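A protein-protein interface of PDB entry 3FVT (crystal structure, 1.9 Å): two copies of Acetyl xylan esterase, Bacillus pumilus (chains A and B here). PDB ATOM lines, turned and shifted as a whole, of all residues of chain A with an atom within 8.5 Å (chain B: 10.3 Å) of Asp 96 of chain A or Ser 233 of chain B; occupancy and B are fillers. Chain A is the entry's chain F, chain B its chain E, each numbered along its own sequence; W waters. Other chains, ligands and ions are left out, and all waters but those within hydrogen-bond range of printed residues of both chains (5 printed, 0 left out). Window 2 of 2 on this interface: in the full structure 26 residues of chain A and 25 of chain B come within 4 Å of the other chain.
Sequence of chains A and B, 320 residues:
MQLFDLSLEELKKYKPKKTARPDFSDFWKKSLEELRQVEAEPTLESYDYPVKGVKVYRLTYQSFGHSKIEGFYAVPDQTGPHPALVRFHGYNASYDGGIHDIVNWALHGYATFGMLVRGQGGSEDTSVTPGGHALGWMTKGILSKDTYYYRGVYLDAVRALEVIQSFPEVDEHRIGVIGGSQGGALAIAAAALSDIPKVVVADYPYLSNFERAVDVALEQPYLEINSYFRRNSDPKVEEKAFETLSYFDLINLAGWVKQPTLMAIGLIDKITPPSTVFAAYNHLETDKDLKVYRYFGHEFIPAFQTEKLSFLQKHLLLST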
ATOM      1  N   TYR A  47      38.637  10.188  12.412  1.00  0.00           N
ATOM      2  CA  TYR A  47      37.794  10.464  11.267  1.00  0.00           C
ATOM      3  C   TYR A  47      37.037  11.754  11.515  1.00  0.00           C
ATOM      4  O   TYR A  47      36.287  11.861  12.481  1.00  0.00           O
ATOM      5  CB  TYR A  47      36.815   9.314  11.055  1.00  0.00           C
ATOM      6  CG  TYR A  47      36.058   9.392   9.759  1.00  0.00           C
ATOM      7  CD1 TYR A  47      36.651   8.992   8.563  1.00  0.00           C
ATOM      8  CD2 TYR A  47      34.741   9.860   9.721  1.00  0.00           C
ATOM      9  CE1 TYR A  47      35.954   9.046   7.363  1.00  0.00           C
ATOM     10  CE2 TYR A  47      34.035   9.923   8.527  1.00  0.00           C
ATOM     11  CZ  TYR A  47      34.646   9.508   7.352  1.00  0.00           C
ATOM     12  OH  TYR A  47      33.937   9.491   6.172  1.00  0.00           O
ATOM     13  N   TYR A  49      34.344  14.592  11.578  1.00  0.00           N
ATOM     14  CA  TYR A  49      32.893  14.587  11.537  1.00  0.00           C
ATOM     15  C   TYR A  49      32.403  15.878  12.157  1.00  0.00           C
ATOM     16  O   TYR A  49      33.004  16.382  13.105  1.00  0.00           O
ATOM     17  CB  TYR A  49      32.345  13.370  12.297  1.00  0.00           C
ATOM     18  CG  TYR A  49      30.848  13.183  12.149  1.00  0.00           C
ATOM     19  CD1 TYR A  49      29.967  13.827  13.008  1.00  0.00           C
ATOM     20  CD2 TYR A  49      30.313  12.411  11.104  1.00  0.00           C
ATOM     21  CE1 TYR A  49      28.584  13.724  12.845  1.00  0.00           C
ATOM     22  CE2 TYR A  49      28.936  12.299  10.931  1.00  0.00           C
ATOM     23  CZ  TYR A  49      28.072  12.955  11.809  1.00  0.00           C
ATOM     24  OH  TYR A  49      26.701  12.808  11.714  1.00  0.00           O
ATOM     25  N   ARG A  58      37.922   5.263  12.496  1.00  0.00           N
ATOM     26  CA  ARG A  58      37.647   4.189  11.573  1.00  0.00           C
ATOM     27  C   ARG A  58      38.485   3.086  12.214  1.00  0.00           C
ATOM     28  O   ARG A  58      39.718   3.170  12.252  1.00  0.00           O
ATOM     29  CB  ARG A  58      38.170   4.518  10.182  1.00  0.00           C
ATOM     30  CG  ARG A  58      37.850   3.446   9.170  1.00  0.00           C
ATOM     31  CD  ARG A  58      36.354   3.301   8.990  1.00  0.00           C
ATOM     32  NE  ARG A  58      36.070   2.285   7.986  1.00  0.00           N
ATOM     33  CZ  ARG A  58      34.923   2.175   7.322  1.00  0.00           C
ATOM     34  NH1 ARG A  58      33.918   3.022   7.545  1.00  0.00           N
ATOM     35  NH2 ARG A  58      34.795   1.212   6.420  1.00  0.00           N
ATOM     36  N   GLY A  71      34.682  -0.532  10.642  1.00  0.00           N
ATOM     37  CA  GLY A  71      33.473   0.142  11.053  1.00  0.00           C
ATOM     38  C   GLY A  71      33.823   1.411  11.790  1.00  0.00           C
ATOM     39  O   GLY A  71      34.958   1.580  12.227  1.00  0.00           O
ATOM     40  N   PHE A  72      32.861   2.313  11.905  1.00  0.00           N
ATOM     41  CA  PHE A  72      33.102   3.547  12.634  1.00  0.00           C
ATOM     42  C   PHE A  72      32.997   3.318  14.132  1.00  0.00           C
ATOM     43  O   PHE A  72      32.115   2.595  14.583  1.00  0.00           O
ATOM     44  CB  PHE A  72      32.086   4.612  12.222  1.00  0.00           C
ATOM     45  CG  PHE A  72      32.309   5.130  10.840  1.00  0.00           C
ATOM     46  CD1 PHE A  72      31.479   4.737   9.794  1.00  0.00           C
ATOM     47  CD2 PHE A  72      33.398   5.945  10.568  1.00  0.00           C
ATOM     48  CE1 PHE A  72      31.742   5.150   8.497  1.00  0.00           C
ATOM     49  CE2 PHE A  72      33.670   6.362   9.275  1.00  0.00           C
ATOM     50  CZ  PHE A  72      32.836   5.959   8.233  1.00  0.00           C
ATOM     51  N   ALA A  93      21.419  -3.137   4.310  1.00  0.00           N
ATOM     52  CA  ALA A  93      20.849  -1.846   4.739  1.00  0.00           C
ATOM     53  C   ALA A  93      21.787  -0.831   5.399  1.00  0.00           C
ATOM     54  O   ALA A  93      21.367  -0.032   6.239  1.00  0.00           O
ATOM     55  CB  ALA A  93      19.666  -2.090   5.641  1.00  0.00           C
ATOM     56  N   SER A  94      23.046  -0.841   5.007  1.00  0.00           N
ATOM     57  CA  SER A  94      24.011   0.074   5.583  1.00  0.00           C
ATOM     58  C   SER A  94      24.451   1.141   4.590  1.00  0.00           C
ATOM     59  O   SER A  94      25.052   0.831   3.564  1.00  0.00           O
ATOM     60  CB  SER A  94      25.221  -0.719   6.079  1.00  0.00           C
ATOM     61  OG  SER A  94      26.209   0.142   6.612  1.00  0.00           O
ATOM     62  N   TYR A  95      24.155   2.398   4.913  1.00  0.00           N
ATOM     63  CA  TYR A  95      24.517   3.536   4.073  1.00  0.00           C
ATOM     64  C   TYR A  95      25.651   4.333   4.711  1.00  0.00           C
ATOM     65  O   TYR A  95      25.493   4.847   5.817  1.00  0.00           O
ATOM     66  CB  TYR A  95      23.319   4.470   3.893  1.00  0.00           C
ATOM     67  CG  TYR A  95      22.169   3.871   3.124  1.00  0.00           C
ATOM     68  CD1 TYR A  95      21.494   2.737   3.593  1.00  0.00           C
ATOM     69  CD2 TYR A  95      21.764   4.422   1.908  1.00  0.00           C
ATOM     70  CE1 TYR A  95      20.445   2.169   2.854  1.00  0.00           C
ATOM     71  CE2 TYR A  95      20.714   3.864   1.169  1.00  0.00           C
ATOM     72  CZ  TYR A  95      20.065   2.740   1.642  1.00  0.00           C
ATOM     73  OH  TYR A  95      19.056   2.174   0.883  1.00  0.00           O
ATOM     74  N   ASP A  96      26.783   4.441   4.025  1.00  0.00           N
ATOM     75  CA  ASP A  96      27.900   5.213   4.554  1.00  0.00           C
ATOM     76  C   ASP A  96      28.235   4.807   6.000  1.00  0.00           C
ATOM     77  O   ASP A  96      28.526   5.643   6.879  1.00  0.00           O
ATOM     78  CB  ASP A  96      27.568   6.709   4.454  1.00  0.00           C
ATOM     79  CG  ASP A  96      27.454   7.186   3.001  1.00  0.00           C
ATOM     80  OD1 ASP A  96      26.830   8.244   2.757  1.00  0.00           O
ATOM     81  OD2 ASP A  96      28.009   6.515   2.107  1.00  0.00           O
ATOM     82  N   GLY A  97      28.175   3.501   6.231  1.00  0.00           N
ATOM     83  CA  GLY A  97      28.495   2.954   7.534  1.00  0.00           C
ATOM     84  C   GLY A  97      27.574   3.288   8.695  1.00  0.00           C
ATOM     85  O   GLY A  97      27.919   2.971   9.826  1.00  0.00           O
ATOM     86  N   GLY A  98      26.410   3.890   8.436  1.00  0.00           N
ATOM     87  CA  GLY A  98      25.506   4.248   9.522  1.00  0.00           C
ATOM     88  C   GLY A  98      26.172   5.212  10.493  1.00  0.00           C
ATOM     89  O   GLY A  98      25.803   5.286  11.667  1.00  0.00           O
ATOM     90  N   ILE A  99      27.140   5.979   9.993  1.00  0.00           N
ATOM     91  CA  ILE A  99      27.906   6.906  10.827  1.00  0.00           C
ATOM     92  C   ILE A  99      27.074   7.882  11.649  1.00  0.00           C
ATOM     93  O   ILE A  99      27.363   8.129  12.819  1.00  0.00           O
ATOM     94  CB  ILE A  99      28.978   7.675   9.967  1.00  0.00           C
ATOM     95  CG1 ILE A  99      29.935   8.441  10.890  1.00  0.00           C
ATOM     96  CG2 ILE A  99      28.300   8.599   8.942  1.00  0.00           C
ATOM     97  CD1 ILE A  99      31.167   8.980  10.179  1.00  0.00           C
ATOM     98  N   HIS A 100      26.004   8.408  11.061  1.00  0.00           N
ATOM     99  CA  HIS A 100      25.170   9.361  11.769  1.00  0.00           C
ATOM    100  C   HIS A 100      24.525   8.732  13.009  1.00  0.00           C
ATOM    101  O   HIS A 100      24.462   9.352  14.055  1.00  0.00           O
ATOM    102  CB  HIS A 100      24.141   9.930  10.799  1.00  0.00           C
ATOM    103  CG  HIS A 100      24.765  10.472   9.552  1.00  0.00           C
ATOM    104  ND1 HIS A 100      25.493  11.640   9.541  1.00  0.00           N
ATOM    105  CD2 HIS A 100      24.855   9.962   8.305  1.00  0.00           C
ATOM    106  CE1 HIS A 100      26.006  11.826   8.339  1.00  0.00           C
ATOM    107  NE2 HIS A 100      25.636  10.822   7.570  1.00  0.00           N
ATOM    108  N   ASP A 101      24.103   7.480  12.914  1.00  0.00           N
ATOM    109  CA  ASP A 101      23.509   6.840  14.076  1.00  0.00           C
ATOM    110  C   ASP A 101      24.572   6.460  15.082  1.00  0.00           C
ATOM    111  O   ASP A 101      24.317   6.438  16.283  1.00  0.00           O
ATOM    112  CB  ASP A 101      22.719   5.606  13.663  1.00  0.00           C
ATOM    113  CG  ASP A 101      21.524   5.957  12.816  1.00  0.00           C
ATOM    114  OD1 ASP A 101      20.676   6.739  13.303  1.00  0.00           O
ATOM    115  OD2 ASP A 101      21.447   5.469  11.670  1.00  0.00           O
ATOM    116  N   ILE A 102      25.769   6.177  14.591  1.00  0.00           N
ATOM    117  CA  ILE A 102      26.868   5.788  15.467  1.00  0.00           C
ATOM    118  C   ILE A 102      27.273   6.976  16.330  1.00  0.00           C
ATOM    119  O   ILE A 102      27.505   6.828  17.532  1.00  0.00           O
ATOM    120  CB  ILE A 102      28.090   5.275  14.636  1.00  0.00           C
ATOM    121  CG1 ILE A 102      27.686   4.001  13.882  1.00  0.00           C
ATOM    122  CG2 ILE A 102      29.303   5.015  15.541  1.00  0.00           C
ATOM    123  CD1 ILE A 102      26.993   2.978  14.744  1.00  0.00           C
ATOM    124  N   GLY A 114      30.115   0.480  15.026  1.00  0.00           N
ATOM    125  CA  GLY A 114      29.139  -0.078  14.099  1.00  0.00           C
ATOM    126  C   GLY A 114      29.869  -1.058  13.200  1.00  0.00           C
ATOM    127  O   GLY A 114      30.488  -0.635  12.220  1.00  0.00           O
ATOM    128  N   LEU A 116      30.569  -3.401  10.335  1.00  0.00           N
ATOM    129  CA  LEU A 116      30.031  -3.531   8.994  1.00  0.00           C
ATOM    130  C   LEU A 116      30.093  -5.021   8.635  1.00  0.00           C
ATOM    131  O   LEU A 116      31.109  -5.694   8.835  1.00  0.00           O
ATOM    132  CB  LEU A 116      30.853  -2.637   8.046  1.00  0.00           C
ATOM    133  CG  LEU A 116      30.810  -1.152   8.477  1.00  0.00           C
ATOM    134  CD1 LEU A 116      31.690  -0.288   7.600  1.00  0.00           C
ATOM    135  CD2 LEU A 116      29.373  -0.631   8.400  1.00  0.00           C
ATOM    136  N   GLN A 120      28.758  -6.355   2.811  1.00  0.00           N
ATOM    137  CA  GLN A 120      27.516  -5.585   2.727  1.00  0.00           C
ATOM    138  C   GLN A 120      27.800  -4.110   2.942  1.00  0.00           C
ATOM    139  O   GLN A 120      28.085  -3.384   1.993  1.00  0.00           O
ATOM    140  CB  GLN A 120      26.522  -6.053   3.779  1.00  0.00           C
ATOM    141  CG  GLN A 120      25.971  -7.438   3.551  1.00  0.00           C
ATOM    142  CD  GLN A 120      24.996  -7.839   4.637  1.00  0.00           C
ATOM    143  OE1 GLN A 120      24.257  -7.002   5.188  1.00  0.00           O
ATOM    144  NE2 GLN A 120      24.970  -9.116   4.942  1.00  0.00           N
ATOM    145  N   GLY A 121      27.738  -3.678   4.201  1.00  0.00           N
ATOM    146  CA  GLY A 121      27.989  -2.279   4.510  1.00  0.00           C
ATOM    147  C   GLY A 121      29.458  -1.958   4.407  1.00  0.00           C
ATOM    148  O   GLY A 121      29.858  -0.792   4.347  1.00  0.00           O
ATOM    149  N   GLY A 122      30.268  -3.012   4.379  1.00  0.00           N
ATOM    150  CA  GLY A 122      31.709  -2.849   4.298  1.00  0.00           C
ATOM    151  C   GLY A 122      32.357  -4.134   4.771  1.00  0.00           C
ATOM    152  O   GLY A 122      31.694  -5.166   4.840  1.00  0.00           O
ATOM    153  N   GLY B 132      32.510  -3.566   0.980  1.00  0.00           N
ATOM    154  CA  GLY B 132      31.072  -3.480   0.790  1.00  0.00           C
ATOM    155  C   GLY B 132      30.576  -3.220  -0.622  1.00  0.00           C
ATOM    156  O   GLY B 132      31.217  -2.505  -1.402  1.00  0.00           O
ATOM    157  N   HIS B 133      29.437  -3.831  -0.946  1.00  0.00           N
ATOM    158  CA  HIS B 133      28.793  -3.650  -2.244  1.00  0.00           C
ATOM    159  C   HIS B 133      27.276  -3.894  -2.113  1.00  0.00           C
ATOM    160  O   HIS B 133      26.809  -4.417  -1.091  1.00  0.00           O
ATOM    161  CB  HIS B 133      29.427  -4.580  -3.297  1.00  0.00           C
ATOM    162  CG  HIS B 133      29.235  -6.043  -3.046  1.00  0.00           C
ATOM    163  ND1 HIS B 133      28.162  -6.751  -3.542  1.00  0.00           N
ATOM    164  CD2 HIS B 133      30.020  -6.951  -2.417  1.00  0.00           C
ATOM    165  CE1 HIS B 133      28.294  -8.031  -3.236  1.00  0.00           C
ATOM    166  NE2 HIS B 133      29.414  -8.179  -2.554  1.00  0.00           N
ATOM    167  N   LEU B 143      35.665  -1.567  -7.040  1.00  0.00           N
ATOM    168  CA  LEU B 143      36.625  -0.488  -6.820  1.00  0.00           C
ATOM    169  C   LEU B 143      37.978  -0.669  -7.509  1.00  0.00           C
ATOM    170  O   LEU B 143      38.798   0.243  -7.489  1.00  0.00           O
ATOM    171  CB  LEU B 143      36.835  -0.211  -5.317  1.00  0.00           C
ATOM    172  CG  LEU B 143      35.633   0.509  -4.699  1.00  0.00           C
ATOM    173  CD1 LEU B 143      35.858   0.791  -3.206  1.00  0.00           C
ATOM    174  CD2 LEU B 143      35.390   1.809  -5.473  1.00  0.00           C
ATOM    175  N   ILE B 225      24.032  -1.057  -9.594  1.00  0.00           N
ATOM    176  CA  ILE B 225      25.072  -0.034  -9.558  1.00  0.00           C
ATOM    177  C   ILE B 225      24.528   1.213  -8.843  1.00  0.00           C
ATOM    178  O   ILE B 225      25.204   1.767  -7.991  1.00  0.00           O
ATOM    179  CB  ILE B 225      25.549   0.301 -10.973  1.00  0.00           C
ATOM    180  CG1 ILE B 225      26.271  -0.921 -11.564  1.00  0.00           C
ATOM    181  CG2 ILE B 225      26.402   1.543 -10.951  1.00  0.00           C
ATOM    182  CD1 ILE B 225      26.316  -0.907 -13.067  1.00  0.00           C
ATOM    183  N   ASN B 226      23.301   1.628  -9.174  1.00  0.00           N
ATOM    184  CA  ASN B 226      22.659   2.781  -8.527  1.00  0.00           C
ATOM    185  C   ASN B 226      22.584   2.490  -7.013  1.00  0.00           C
ATOM    186  O   ASN B 226      22.913   3.347  -6.181  1.00  0.00           O
ATOM    187  CB  ASN B 226      21.237   2.988  -9.090  1.00  0.00           C
ATOM    188  CG  ASN B 226      21.232   3.192 -10.613  1.00  0.00           C
ATOM    189  OD1 ASN B 226      21.784   2.382 -11.342  1.00  0.00           O
ATOM    190  ND2 ASN B 226      20.598   4.265 -11.087  1.00  0.00           N
ATOM    191  N   SER B 227      22.124   1.286  -6.666  1.00  0.00           N
ATOM    192  CA  SER B 227      22.016   0.889  -5.264  1.00  0.00           C
ATOM    193  C   SER B 227      23.361   1.067  -4.578  1.00  0.00           C
ATOM    194  O   SER B 227      23.447   1.572  -3.466  1.00  0.00           O
ATOM    195  CB  SER B 227      21.597  -0.577  -5.163  1.00  0.00           C
ATOM    196  OG  SER B 227      20.388  -0.811  -5.864  1.00  0.00           O
ATOM    197  N   TYR B 228      24.413   0.623  -5.254  1.00  0.00           N
ATOM    198  CA  TYR B 228      25.767   0.737  -4.735  1.00  0.00           C
ATOM    199  C   TYR B 228      26.115   2.191  -4.362  1.00  0.00           C
ATOM    200  O   TYR B 228      26.574   2.484  -3.235  1.00  0.00           O
ATOM    201  CB  TYR B 228      26.755   0.208  -5.775  1.00  0.00           C
ATOM    202  CG  TYR B 228      28.204   0.320  -5.360  1.00  0.00           C
ATOM    203  CD1 TYR B 228      28.750  -0.536  -4.408  1.00  0.00           C
ATOM    204  CD2 TYR B 228      29.028   1.289  -5.929  1.00  0.00           C
ATOM    205  CE1 TYR B 228      30.084  -0.428  -4.036  1.00  0.00           C
ATOM    206  CE2 TYR B 228      30.350   1.410  -5.574  1.00  0.00           C
ATOM    207  CZ  TYR B 228      30.878   0.555  -4.632  1.00  0.00           C
ATOM    208  OH  TYR B 228      32.194   0.672  -4.305  1.00  0.00           O
ATOM    209  N   PHE B 229      25.892   3.104  -5.306  1.00  0.00           N
ATOM    210  CA  PHE B 229      26.181   4.511  -5.067  1.00  0.00           C
ATOM    211  C   PHE B 229      25.365   5.093  -3.922  1.00  0.00           C
ATOM    212  O   PHE B 229      25.840   5.974  -3.219  1.00  0.00           O
ATOM    213  CB  PHE B 229      25.939   5.364  -6.329  1.00  0.00           C
ATOM    214  CG  PHE B 229      26.824   5.011  -7.488  1.00  0.00           C
ATOM    215  CD1 PHE B 229      28.098   4.466  -7.280  1.00  0.00           C
ATOM    216  CD2 PHE B 229      26.383   5.202  -8.789  1.00  0.00           C
ATOM    217  CE1 PHE B 229      28.917   4.114  -8.360  1.00  0.00           C
ATOM    218  CE2 PHE B 229      27.197   4.851  -9.884  1.00  0.00           C
ATOM    219  CZ  PHE B 229      28.466   4.305  -9.668  1.00  0.00           C
ATOM    220  N   ARG B 230      24.134   4.624  -3.735  1.00  0.00           N
ATOM    221  CA  ARG B 230      23.322   5.143  -2.645  1.00  0.00           C
ATOM    222  C   ARG B 230      23.947   4.799  -1.287  1.00  0.00           C
ATOM    223  O   ARG B 230      23.879   5.578  -0.341  1.00  0.00           O
ATOM    224  CB  ARG B 230      21.900   4.563  -2.711  1.00  0.00           C
ATOM    225  CG  ARG B 230      21.039   5.079  -3.879  1.00  0.00           C
ATOM    226  CD  ARG B 230      19.756   4.250  -4.050  1.00  0.00           C
ATOM    227  NE  ARG B 230      19.005   4.117  -2.806  1.00  0.00           N
ATOM    228  CZ  ARG B 230      18.157   5.030  -2.330  1.00  0.00           C
ATOM    229  NH1 ARG B 230      17.937   6.156  -3.000  1.00  0.00           N
ATOM    230  NH2 ARG B 230      17.539   4.822  -1.163  1.00  0.00           N
ATOM    231  N   ARG B 231      24.577   3.636  -1.213  1.00  0.00           N
ATOM    232  CA  ARG B 231      25.168   3.151   0.032  1.00  0.00           C
ATOM    233  C   ARG B 231      26.606   3.611   0.268  1.00  0.00           C
ATOM    234  O   ARG B 231      27.116   3.538   1.389  1.00  0.00           O
ATOM    235  CB  ARG B 231      25.097   1.627   0.045  1.00  0.00           C
ATOM    236  CG  ARG B 231      23.668   1.106   0.181  1.00  0.00           C
ATOM    237  CD  ARG B 231      23.520  -0.361  -0.241  1.00  0.00           C
ATOM    238  NE  ARG B 231      22.190  -0.876   0.119  1.00  0.00           N
ATOM    239  CZ  ARG B 231      21.062  -0.563  -0.508  1.00  0.00           C
ATOM    240  NH1 ARG B 231      21.075   0.260  -1.555  1.00  0.00           N
ATOM    241  NH2 ARG B 231      19.902  -1.037  -0.059  1.00  0.00           N
ATOM    242  N   ASN B 232      27.242   4.090  -0.794  1.00  0.00           N
ATOM    243  CA  ASN B 232      28.620   4.578  -0.745  1.00  0.00           C
ATOM    244  C   ASN B 232      28.621   5.894  -1.535  1.00  0.00           C
ATOM    245  O   ASN B 232      28.875   5.895  -2.741  1.00  0.00           O
ATOM    246  CB  ASN B 232      29.533   3.535  -1.386  1.00  0.00           C
ATOM    247  CG  ASN B 232      29.263   2.138  -0.856  1.00  0.00           C
ATOM    248  OD1 ASN B 232      28.445   1.386  -1.406  1.00  0.00           O
ATOM    249  ND2 ASN B 232      29.924   1.795   0.235  1.00  0.00           N
ATOM    250  N   SER B 233      28.350   6.992  -0.825  1.00  0.00           N
ATOM    251  CA  SER B 233      28.196   8.326  -1.411  1.00  0.00           C
ATOM    252  C   SER B 233      29.414   9.182  -1.772  1.00  0.00           C
ATOM    253  O   SER B 233      29.247  10.275  -2.306  1.00  0.00           O
ATOM    254  CB  SER B 233      27.270   9.149  -0.508  1.00  0.00           C
ATOM    255  OG  SER B 233      27.908   9.446   0.727  1.00  0.00           O
ATOM    256  N   ASP B 234      30.623   8.726  -1.468  1.00  0.00           N
ATOM    257  CA  ASP B 234      31.819   9.501  -1.819  1.00  0.00           C
ATOM    258  C   ASP B 234      31.857   9.661  -3.342  1.00  0.00           C
ATOM    259  O   ASP B 234      31.794   8.666  -4.074  1.00  0.00           O
ATOM    260  CB  ASP B 234      33.083   8.777  -1.336  1.00  0.00           C
ATOM    261  CG  ASP B 234      34.374   9.513  -1.703  1.00  0.00           C
ATOM    262  OD1 ASP B 234      34.334  10.738  -1.949  1.00  0.00           O
ATOM    263  OD2 ASP B 234      35.442   8.856  -1.730  1.00  0.00           O
ATOM    264  N   PRO B 235      31.930  10.915  -3.842  1.00  0.00           N
ATOM    265  CA  PRO B 235      31.970  11.142  -5.294  1.00  0.00           C
ATOM    266  C   PRO B 235      33.095  10.373  -6.000  1.00  0.00           C
ATOM    267  O   PRO B 235      32.936   9.914  -7.138  1.00  0.00           O
ATOM    268  CB  PRO B 235      32.144  12.659  -5.400  1.00  0.00           C
ATOM    269  CG  PRO B 235      31.381  13.150  -4.228  1.00  0.00           C
ATOM    270  CD  PRO B 235      31.829  12.200  -3.126  1.00  0.00           C
ATOM    271  N   LYS B 236      34.229  10.240  -5.318  1.00  0.00           N
ATOM    272  CA  LYS B 236      35.386   9.538  -5.879  1.00  0.00           C
ATOM    273  C   LYS B 236      35.110   8.050  -6.039  1.00  0.00           C
ATOM    274  O   LYS B 236      35.736   7.379  -6.846  1.00  0.00           O
ATOM    275  CB  LYS B 236      36.622   9.742  -4.995  1.00  0.00           C
ATOM    276  CG  LYS B 236      37.146  11.167  -4.958  1.00  0.00           C
ATOM    277  CD  LYS B 236      38.266  11.281  -3.931  1.00  0.00           C
ATOM    278  CE  LYS B 236      38.835  12.688  -3.878  1.00  0.00           C
ATOM    279  NZ  LYS B 236      40.068  12.715  -3.031  1.00  0.00           N
ATOM    280  N   VAL B 237      34.180   7.528  -5.258  1.00  0.00           N
ATOM    281  CA  VAL B 237      33.826   6.115  -5.373  1.00  0.00           C
ATOM    282  C   VAL B 237      33.104   5.923  -6.706  1.00  0.00           C
ATOM    283  O   VAL B 237      33.331   4.941  -7.405  1.00  0.00           O
ATOM    284  CB  VAL B 237      32.888   5.684  -4.230  1.00  0.00           C
ATOM    285  CG1 VAL B 237      32.015   4.516  -4.672  1.00  0.00           C
ATOM    286  CG2 VAL B 237      33.723   5.275  -3.011  1.00  0.00           C
ATOM    287  N   GLU B 238      32.232   6.875  -7.046  1.00  0.00           N
ATOM    288  CA  GLU B 238      31.462   6.800  -8.291  1.00  0.00           C
ATOM    289  C   GLU B 238      32.393   6.910  -9.477  1.00  0.00           C
ATOM    290  O   GLU B 238      32.259   6.187 -10.479  1.00  0.00           O
ATOM    291  CB  GLU B 238      30.401   7.909  -8.357  1.00  0.00           C
ATOM    292  CG  GLU B 238      29.490   7.779  -9.575  1.00  0.00           C
ATOM    293  CD  GLU B 238      28.330   8.763  -9.573  1.00  0.00           C
ATOM    294  OE1 GLU B 238      28.116   9.433  -8.539  1.00  0.00           O
ATOM    295  OE2 GLU B 238      27.623   8.849 -10.606  1.00  0.00           O
ATOM    296  N   GLU B 239      33.331   7.841  -9.370  1.00  0.00           N
ATOM    297  CA  GLU B 239      34.320   8.028 -10.407  1.00  0.00           C
ATOM    298  C   GLU B 239      35.059   6.706 -10.619  1.00  0.00           C
ATOM    299  O   GLU B 239      35.138   6.192 -11.735  1.00  0.00           O
ATOM    300  CB  GLU B 239      35.327   9.108  -9.994  1.00  0.00           C
ATOM    301  CG  GLU B 239      34.770  10.507  -9.932  1.00  0.00           C
ATOM    302  CD  GLU B 239      35.849  11.543  -9.631  1.00  0.00           C
ATOM    303  OE1 GLU B 239      35.527  12.756  -9.638  1.00  0.00           O
ATOM    304  OE2 GLU B 239      37.018  11.146  -9.389  1.00  0.00           O
HETATM  305  O   HOH W   1      28.067   1.399   2.067  1.00  0.00           O
HETATM  306  O   HOH W   2      27.818  -1.198  -0.053  1.00  0.00           O
HETATM  307  O   HOH W   3      17.272   0.907  -0.514  1.00  0.00           O
HETATM  308  O   HOH W   4      24.579   7.119   1.660  1.00  0.00           O
HETATM  309  O   HOH W   5      24.962  -3.800   1.031  1.00  0.00           O
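The guanidinium group (NH2) of Arg 231 of chain B lies within hydrogen-bond range of the side-chain hydroxyl (OH) of Tyr 95 of chain A.
O of Arg 231 of chain B sits at hydrogen-bond distance from N of Asp 96 of chain A.
O of Gln 120 of chain A sits at hydrogen-bond distance from N of His 133 of chain B (3.3 Å).
OG of Ser 233 of chain B sits at hydrogen-bond distance from OD1 of Asp 96 of chain A, at 2.6 Å.
Among the printed residues, merely in contact across the chains: Ser 94 of chain A with Arg 231 of chain B (3.6 Å), Tyr 95 of chain A with Arg 230 of chain B (3.3 Å), Asp 96 of chain A with Asn 232 of chain B (3.5 Å), Gln 120 of chain A with Gly 132 of chain B (3.2 Å) and Gly 122 of chain A with Gly 132 of chain B (3.5 Å).
Of the 18 printed residues of chain B, 6 touch a printed residue of chain A.
Among the printed residues, 9 pairs touch across the chains.
Among the printed residues, no Asp or Glu carboxylate lies within 4 Å of a Lys or Arg side-chain nitrogen of the other chain.
Water W3 bridges OH of Tyr 95 of chain A and NH2 of Arg 231 of chain B.
Water W5 bridges the backbone carbonyl oxygen of His 133 of chain B (2.9 Å) and the backbone carbonyl oxygen of Gln 120 of chain A (3.3 Å).
No position is printed for both chains.
Of the 9 pairs that touch across the chains among the printed residues, none has its exchanged pair printed and touching as well.
Printed residues of chain B within 4 Å of Tyr 95 of chain A: Arg 230 (3.3 Å) and Arg 231 (3.5 Å).
No residue of chain B comes within 4 Å of Gly 97 of chain A.
Printed residues of chain A within 4 Å of Gly 132 of chain B: Gln 120 (3.2 Å) and Gly 122 (3.5 Å).
Of the printed residues of chain A, His 133 of chain B touches Gln 120.
Printed residues of chain A within 4 Å of Asn 232 of chain B: Asp 96 (3.5 Å).
Of chain A, only Asp 96 (2.6 Å) comes within 4 Å of Ser 233 of chain B.
Glu 238 of chain B touches none of the printed residues of chain A.
The nearest residue of chain A that does not touch Ser 233 of chain B is Tyr 95 of chain A (6.7 Å).
The nearest printed residue of chain A that does not touch Arg 231 of chain B is Ala 93 of chain A (4.8 Å).
The side-chain amide oxygen of Asn 232 of chain B lies close to the backbone carbonyl oxygen of Tyr 228 of chain B (2.8 Å).
O of Ser 227 of chain B lies within hydrogen-bond range of NH1 of Arg 231 of chain B.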
